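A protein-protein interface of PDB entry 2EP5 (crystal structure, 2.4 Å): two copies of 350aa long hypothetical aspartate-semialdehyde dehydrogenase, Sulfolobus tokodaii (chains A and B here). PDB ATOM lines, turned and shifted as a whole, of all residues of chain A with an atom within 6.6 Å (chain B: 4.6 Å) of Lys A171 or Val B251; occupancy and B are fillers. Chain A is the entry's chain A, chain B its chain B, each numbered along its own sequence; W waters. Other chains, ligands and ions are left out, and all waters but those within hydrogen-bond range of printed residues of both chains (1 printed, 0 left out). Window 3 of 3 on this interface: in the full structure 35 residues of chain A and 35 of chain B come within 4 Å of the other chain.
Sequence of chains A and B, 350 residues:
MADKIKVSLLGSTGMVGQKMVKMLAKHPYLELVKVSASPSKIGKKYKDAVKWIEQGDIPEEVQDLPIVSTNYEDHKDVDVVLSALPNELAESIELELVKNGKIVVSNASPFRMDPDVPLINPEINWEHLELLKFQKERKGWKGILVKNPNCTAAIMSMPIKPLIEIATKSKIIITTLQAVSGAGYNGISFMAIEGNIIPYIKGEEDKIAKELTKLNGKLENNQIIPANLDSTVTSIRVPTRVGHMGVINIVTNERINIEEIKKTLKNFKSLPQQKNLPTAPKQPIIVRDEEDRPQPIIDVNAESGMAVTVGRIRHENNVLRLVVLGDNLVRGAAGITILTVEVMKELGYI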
ATOM      1  N   ILE A 166      -5.932 -17.192  21.191  1.00  0.00           N
ATOM      2  CA  ILE A 166      -6.260 -18.283  20.281  1.00  0.00           C
ATOM      3  C   ILE A 166      -5.581 -19.554  20.780  1.00  0.00           C
ATOM      4  O   ILE A 166      -6.214 -20.611  20.886  1.00  0.00           O
ATOM      5  CB  ILE A 166      -5.761 -17.992  18.857  1.00  0.00           C
ATOM      6  CG1 ILE A 166      -6.391 -16.698  18.343  1.00  0.00           C
ATOM      7  CG2 ILE A 166      -6.108 -19.149  17.939  1.00  0.00           C
ATOM      8  CD1 ILE A 166      -5.861 -16.258  16.988  1.00  0.00           C
ATOM      9  N   ALA A 167      -4.294 -19.429  21.095  1.00  0.00           N
ATOM     10  CA  ALA A 167      -3.486 -20.548  21.582  1.00  0.00           C
ATOM     11  C   ALA A 167      -4.038 -21.155  22.869  1.00  0.00           C
ATOM     12  O   ALA A 167      -3.940 -22.363  23.088  1.00  0.00           O
ATOM     13  CB  ALA A 167      -2.038 -20.090  21.800  1.00  0.00           C
ATOM     14  N   THR A 168      -4.610 -20.317  23.722  1.00  0.00           N
ATOM     15  CA  THR A 168      -5.170 -20.790  24.985  1.00  0.00           C
ATOM     16  C   THR A 168      -6.368 -21.714  24.769  1.00  0.00           C
ATOM     17  O   THR A 168      -6.588 -22.650  25.540  1.00  0.00           O
ATOM     18  CB  THR A 168      -5.603 -19.607  25.879  1.00  0.00           C
ATOM     19  OG1 THR A 168      -4.437 -18.939  26.384  1.00  0.00           O
ATOM     20  CG2 THR A 168      -6.450 -20.097  27.037  1.00  0.00           C
ATOM     21  N   LYS A 169      -7.138 -21.450  23.719  1.00  0.00           N
ATOM     22  CA  LYS A 169      -8.309 -22.263  23.409  1.00  0.00           C
ATOM     23  C   LYS A 169      -8.007 -23.177  22.225  1.00  0.00           C
ATOM     24  O   LYS A 169      -8.644 -23.071  21.172  1.00  0.00           O
ATOM     25  CB  LYS A 169      -9.501 -21.376  23.047  1.00  0.00           C
ATOM     26  CG  LYS A 169      -9.882 -20.321  24.065  1.00  0.00           C
ATOM     27  CD  LYS A 169     -10.996 -19.465  23.473  1.00  0.00           C
ATOM     28  CE  LYS A 169     -11.304 -18.220  24.288  1.00  0.00           C
ATOM     29  NZ  LYS A 169     -12.195 -17.308  23.507  1.00  0.00           N
ATOM     30  N   SER A 170      -7.042 -24.073  22.390  1.00  0.00           N
ATOM     31  CA  SER A 170      -6.683 -24.976  21.308  1.00  0.00           C
ATOM     32  C   SER A 170      -5.705 -26.036  21.770  1.00  0.00           C
ATOM     33  O   SER A 170      -5.293 -26.065  22.932  1.00  0.00           O
ATOM     34  CB  SER A 170      -6.017 -24.201  20.177  1.00  0.00           C
ATOM     35  OG  SER A 170      -4.683 -23.872  20.539  1.00  0.00           O
ATOM     36  N   LYS A 171      -5.352 -26.912  20.838  1.00  0.00           N
ATOM     37  CA  LYS A 171      -4.366 -27.952  21.083  1.00  0.00           C
ATOM     38  C   LYS A 171      -3.191 -27.477  20.227  1.00  0.00           C
ATOM     39  O   LYS A 171      -3.303 -27.341  19.000  1.00  0.00           O
ATOM     40  CB  LYS A 171      -4.873 -29.322  20.618  1.00  0.00           C
ATOM     41  CG  LYS A 171      -3.838 -30.446  20.689  1.00  0.00           C
ATOM     42  CD  LYS A 171      -3.334 -30.699  22.113  1.00  0.00           C
ATOM     43  CE  LYS A 171      -2.103 -31.610  22.117  1.00  0.00           C
ATOM     44  NZ  LYS A 171      -1.579 -31.878  23.489  1.00  0.00           N
ATOM     45  N   ILE A 172      -2.080 -27.190  20.892  1.00  0.00           N
ATOM     46  CA  ILE A 172      -0.885 -26.691  20.227  1.00  0.00           C
ATOM     47  C   ILE A 172       0.086 -27.789  19.858  1.00  0.00           C
ATOM     48  O   ILE A 172       0.659 -28.427  20.739  1.00  0.00           O
ATOM     49  CB  ILE A 172      -0.136 -25.688  21.129  1.00  0.00           C
ATOM     50  CG1 ILE A 172      -1.026 -24.475  21.396  1.00  0.00           C
ATOM     51  CG2 ILE A 172       1.174 -25.270  20.472  1.00  0.00           C
ATOM     52  CD1 ILE A 172      -0.583 -23.652  22.553  1.00  0.00           C
ATOM     53  N   ILE A 173       0.265 -28.001  18.554  1.00  0.00           N
ATOM     54  CA  ILE A 173       1.204 -28.997  18.059  1.00  0.00           C
ATOM     55  C   ILE A 173       2.434 -28.250  17.549  1.00  0.00           C
ATOM     56  O   ILE A 173       2.324 -27.355  16.704  1.00  0.00           O
ATOM     57  CB  ILE A 173       0.626 -29.814  16.885  1.00  0.00           C
ATOM     58  CG1 ILE A 173      -0.641 -30.565  17.331  1.00  0.00           C
ATOM     59  CG2 ILE A 173       1.690 -30.787  16.370  1.00  0.00           C
ATOM     60  CD1 ILE A 173      -0.399 -31.650  18.374  1.00  0.00           C
ATOM     61  N   ASP A 230      -2.108 -26.341  26.097  1.00  0.00           N
ATOM     62  CA  ASP A 230      -1.985 -27.774  25.939  1.00  0.00           C
ATOM     63  C   ASP A 230      -1.147 -28.011  24.689  1.00  0.00           C
ATOM     64  O   ASP A 230      -1.672 -28.176  23.590  1.00  0.00           O
ATOM     65  CB  ASP A 230      -3.375 -28.410  25.805  1.00  0.00           C
ATOM     66  CG  ASP A 230      -3.312 -29.900  25.525  1.00  0.00           C
ATOM     67  OD1 ASP A 230      -2.327 -30.551  25.943  1.00  0.00           O
ATOM     68  OD2 ASP A 230      -4.252 -30.425  24.892  1.00  0.00           O
ATOM     69  N   SER A 231       0.168 -28.023  24.859  1.00  0.00           N
ATOM     70  CA  SER A 231       1.039 -28.224  23.717  1.00  0.00           C
ATOM     71  C   SER A 231       1.819 -29.529  23.700  1.00  0.00           C
ATOM     72  O   SER A 231       2.285 -30.005  24.732  1.00  0.00           O
ATOM     73  CB  SER A 231       2.003 -27.035  23.581  1.00  0.00           C
ATOM     74  OG  SER A 231       2.403 -26.547  24.847  1.00  0.00           O
ATOM     75  N   THR A 232       1.939 -30.105  22.508  1.00  0.00           N
ATOM     76  CA  THR A 232       2.689 -31.338  22.303  1.00  0.00           C
ATOM     77  C   THR A 232       3.804 -30.963  21.319  1.00  0.00           C
ATOM     78  O   THR A 232       3.546 -30.474  20.215  1.00  0.00           O
ATOM     79  CB  THR A 232       1.784 -32.454  21.719  1.00  0.00           C
ATOM     80  OG1 THR A 232       0.847 -32.868  22.720  1.00  0.00           O
ATOM     81  CG2 THR A 232       2.605 -33.659  21.291  1.00  0.00           C
ATOM     82  N   ASN A 249       1.389 -25.281  15.026  1.00  0.00           N
ATOM     83  CA  ASN A 249       0.034 -25.550  14.564  1.00  0.00           C
ATOM     84  C   ASN A 249      -0.948 -25.369  15.709  1.00  0.00           C
ATOM     85  O   ASN A 249      -0.998 -26.186  16.630  1.00  0.00           O
ATOM     86  CB  ASN A 249      -0.103 -26.972  14.016  1.00  0.00           C
ATOM     87  CG  ASN A 249       0.600 -27.161  12.684  1.00  0.00           C
ATOM     88  OD1 ASN A 249       1.806 -27.390  12.631  1.00  0.00           O
ATOM     89  ND2 ASN A 249      -0.155 -27.051  11.598  1.00  0.00           N
ATOM     90  N   ILE A 250      -1.715 -24.288  15.663  1.00  0.00           N
ATOM     91  CA  ILE A 250      -2.699 -24.046  16.700  1.00  0.00           C
ATOM     92  C   ILE A 250      -4.014 -24.677  16.234  1.00  0.00           C
ATOM     93  O   ILE A 250      -4.770 -24.071  15.467  1.00  0.00           O
ATOM     94  CB  ILE A 250      -2.867 -22.535  16.949  1.00  0.00           C
ATOM     95  CG1 ILE A 250      -1.526 -21.949  17.411  1.00  0.00           C
ATOM     96  CG2 ILE A 250      -3.941 -22.289  17.996  1.00  0.00           C
ATOM     97  CD1 ILE A 250      -1.569 -20.465  17.755  1.00  0.00           C
ATOM     98  N   VAL A 251      -4.258 -25.908  16.686  1.00  0.00           N
ATOM     99  CA  VAL A 251      -5.467 -26.660  16.322  1.00  0.00           C
ATOM    100  C   VAL A 251      -6.663 -26.158  17.115  1.00  0.00           C
ATOM    101  O   VAL A 251      -6.798 -26.446  18.300  1.00  0.00           O
ATOM    102  CB  VAL A 251      -5.289 -28.177  16.597  1.00  0.00           C
ATOM    103  CG1 VAL A 251      -6.462 -28.962  16.011  1.00  0.00           C
ATOM    104  CG2 VAL A 251      -3.958 -28.657  16.006  1.00  0.00           C
ATOM    105  N   THR A 252      -7.542 -25.422  16.446  1.00  0.00           N
ATOM    106  CA  THR A 252      -8.713 -24.855  17.101  1.00  0.00           C
ATOM    107  C   THR A 252      -9.796 -24.469  16.100  1.00  0.00           C
ATOM    108  O   THR A 252      -9.511 -24.248  14.927  1.00  0.00           O
ATOM    109  CB  THR A 252      -8.315 -23.591  17.895  1.00  0.00           C
ATOM    110  OG1 THR A 252      -9.487 -22.966  18.425  1.00  0.00           O
ATOM    111  CG2 THR A 252      -7.571 -22.604  16.990  1.00  0.00           C
ATOM    112  N   SER B 170     -10.130 -37.523  13.759  1.00  0.00           N
ATOM    113  CA  SER B 170      -9.155 -36.600  14.338  1.00  0.00           C
ATOM    114  C   SER B 170      -8.602 -35.612  13.326  1.00  0.00           C
ATOM    115  O   SER B 170      -8.762 -35.785  12.117  1.00  0.00           O
ATOM    116  CB  SER B 170      -7.969 -37.378  14.891  1.00  0.00           C
ATOM    117  OG  SER B 170      -7.188 -37.877  13.817  1.00  0.00           O
ATOM    118  N   LYS B 171      -7.948 -34.573  13.835  1.00  0.00           N
ATOM    119  CA  LYS B 171      -7.308 -33.596  12.968  1.00  0.00           C
ATOM    120  C   LYS B 171      -5.874 -34.100  12.858  1.00  0.00           C
ATOM    121  O   LYS B 171      -5.212 -34.297  13.870  1.00  0.00           O
ATOM    122  CB  LYS B 171      -7.328 -32.200  13.588  1.00  0.00           C
ATOM    123  CG  LYS B 171      -6.527 -31.173  12.780  1.00  0.00           C
ATOM    124  CD  LYS B 171      -7.062 -30.995  11.350  1.00  0.00           C
ATOM    125  CE  LYS B 171      -6.154 -30.068  10.525  1.00  0.00           C
ATOM    126  NZ  LYS B 171      -6.720 -29.658   9.203  1.00  0.00           N
ATOM    127  N   ASN B 249       1.035 -36.130  14.033  1.00  0.00           N
ATOM    128  CA  ASN B 249       0.269 -35.913  15.252  1.00  0.00           C
ATOM    129  C   ASN B 249      -1.225 -36.087  14.971  1.00  0.00           C
ATOM    130  O   ASN B 249      -1.844 -35.281  14.269  1.00  0.00           O
ATOM    131  CB  ASN B 249       0.504 -34.507  15.826  1.00  0.00           C
ATOM    132  CG  ASN B 249       1.913 -34.319  16.388  1.00  0.00           C
ATOM    133  OD1 ASN B 249       2.850 -33.963  15.662  1.00  0.00           O
ATOM    134  ND2 ASN B 249       2.067 -34.567  17.683  1.00  0.00           N
ATOM    135  N   ILE B 250      -1.795 -37.155  15.512  1.00  0.00           N
ATOM    136  CA  ILE B 250      -3.214 -37.419  15.344  1.00  0.00           C
ATOM    137  C   ILE B 250      -3.895 -36.860  16.592  1.00  0.00           C
ATOM    138  O   ILE B 250      -3.826 -37.456  17.675  1.00  0.00           O
ATOM    139  CB  ILE B 250      -3.462 -38.932  15.204  1.00  0.00           C
ATOM    140  CG1 ILE B 250      -2.772 -39.432  13.926  1.00  0.00           C
ATOM    141  CG2 ILE B 250      -4.972 -39.230  15.187  1.00  0.00           C
ATOM    142  CD1 ILE B 250      -2.779 -40.941  13.736  1.00  0.00           C
ATOM    143  N   VAL B 251      -4.513 -35.690  16.438  1.00  0.00           N
ATOM    144  CA  VAL B 251      -5.202 -35.015  17.535  1.00  0.00           C
ATOM    145  C   VAL B 251      -6.662 -35.442  17.598  1.00  0.00           C
ATOM    146  O   VAL B 251      -7.478 -35.006  16.787  1.00  0.00           O
ATOM    147  CB  VAL B 251      -5.151 -33.481  17.368  1.00  0.00           C
ATOM    148  CG1 VAL B 251      -5.828 -32.802  18.563  1.00  0.00           C
ATOM    149  CG2 VAL B 251      -3.701 -33.021  17.231  1.00  0.00           C
ATOM    150  N   THR B 252      -6.983 -36.282  18.579  1.00  0.00           N
ATOM    151  CA  THR B 252      -8.339 -36.801  18.745  1.00  0.00           C
ATOM    152  C   THR B 252      -8.680 -37.074  20.211  1.00  0.00           C
ATOM    153  O   THR B 252      -7.827 -36.977  21.089  1.00  0.00           O
ATOM    154  CB  THR B 252      -8.505 -38.124  17.972  1.00  0.00           C
ATOM    155  OG1 THR B 252      -9.833 -38.632  18.160  1.00  0.00           O
ATOM    156  CG2 THR B 252      -7.495 -39.159  18.470  1.00  0.00           C
ATOM    157  N   ASN B 317      -2.075 -35.625  25.888  1.00  0.00           N
ATOM    158  CA  ASN B 317      -3.462 -35.198  25.913  1.00  0.00           C
ATOM    159  C   ASN B 317      -4.073 -34.914  24.540  1.00  0.00           C
ATOM    160  O   ASN B 317      -3.691 -33.962  23.859  1.00  0.00           O
ATOM    161  CB  ASN B 317      -3.620 -33.968  26.812  1.00  0.00           C
ATOM    162  CG  ASN B 317      -5.064 -33.507  26.906  1.00  0.00           C
ATOM    163  OD1 ASN B 317      -5.953 -34.295  27.243  1.00  0.00           O
ATOM    164  ND2 ASN B 317      -5.309 -32.232  26.603  1.00  0.00           N
ATOM    165  N   ASN B 318      -5.032 -35.748  24.147  1.00  0.00           N
ATOM    166  CA  ASN B 318      -5.728 -35.593  22.871  1.00  0.00           C
ATOM    167  C   ASN B 318      -4.839 -35.678  21.641  1.00  0.00           C
ATOM    168  O   ASN B 318      -5.135 -35.051  20.619  1.00  0.00           O
ATOM    169  CB  ASN B 318      -6.476 -34.257  22.837  1.00  0.00           C
ATOM    170  CG  ASN B 318      -7.610 -34.202  23.829  1.00  0.00           C
ATOM    171  OD1 ASN B 318      -7.495 -34.698  24.946  1.00  0.00           O
ATOM    172  ND2 ASN B 318      -8.711 -33.580  23.432  1.00  0.00           N
ATOM    173  N   VAL B 319      -3.759 -36.445  21.720  1.00  0.00           N
ATOM    174  CA  VAL B 319      -2.876 -36.564  20.570  1.00  0.00           C
ATOM    175  C   VAL B 319      -1.952 -37.764  20.581  1.00  0.00           C
ATOM    176  O   VAL B 319      -1.307 -38.072  21.585  1.00  0.00           O
ATOM    177  CB  VAL B 319      -1.995 -35.304  20.391  1.00  0.00           C
ATOM    178  CG1 VAL B 319      -1.090 -35.121  21.593  1.00  0.00           C
ATOM    179  CG2 VAL B 319      -1.167 -35.431  19.109  1.00  0.00           C
HETATM  180  O   HOH W   1       4.687 -32.797  18.016  1.00  0.00           O
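Among the printed residues, no Asp or Glu carboxylate lies within 4 Å of a Lys or Arg side-chain nitrogen of the other chain.
Among the printed residues, pairs that only touch across the chains: Lys A171 with Val B251, Lys A171 with Val B319, Ile A173 with Asn B249, Ile A173 with Val B251, Ile A173 with Val B319, Thr A232 with Asn B249, Thr A232 with Val B319 and Val A251 with Lys B171.
Lys A171 touches just these residues of chain B: Val B251, Asn B317 and Val B319.
Val B251 touches two residues of chain A.
Printed residues of chain B within 4 Å of Asp A230: Asn B317 (2.7 Å).
Of the printed residues of chain A, Asn B249 touches Ile A173 (3.5 Å) and Thr A232 (3.8 Å).
Of the printed residues of chain A, Asn B317 touches Lys A171 and Asp A230.
Printed residues of chain A within 4 Å of Lys B171: Val A251 (3.9 Å).
Of the printed residues of chain B, Thr A232 touches Asn B249 (3.8 Å) and Val B319 (3.2 Å).
Ile A250 touches none of the printed residues of chain B.
Ile A166 touches none of the printed residues of chain B.
The nearest printed residue of chain B that does not touch Lys A171 is Asn B318 (4.8 Å).
Lys A171 touches Val B251, and with the chains exchanged Val A251 touches Lys B171.
Positions printed for both chains: 170, 171, 249, 250, 251 and 252.
Of the 10 pairs that touch across the chains among the printed residues, 2 have their exchanged pair printed and touching as well.
The side-chain carboxylate (OD2) of Asp A230 sits at hydrogen-bond distance from the side-chain amide nitrogen (ND2) of Asn B317.
The side-chain amino group (NZ) of Lys A171 sits at hydrogen-bond distance from the backbone carbonyl oxygen (O) of Asn B317 (3.0 Å).
NZ of Lys A171 is in salt-bridge range of OD1 of Asp A230.
OD1 of Asn B318 lies close to OD1 of Asn B317, at 2.8 Å.
The backbone NH (N) of Asn A249 sits at hydrogen-bond distance from the backbone carbonyl oxygen (O) of Ile A173, at 2.8 Å.
N of Val B251 lies within hydrogen-bond range of O of Lys B171, at 3.0 Å.
O of Lys A171 sits at hydrogen-bond distance from N of Val A251.
The side-chain amino group of Lys A171 sits at hydrogen-bond distance from the side-chain hydroxyl of Thr A232 (2.7 Å).
Water W1 bridges the side-chain amide nitrogen of Asn B249 (3.2 Å) and the backbone carbonyl oxygen of Thr A232 (3.4 Å).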
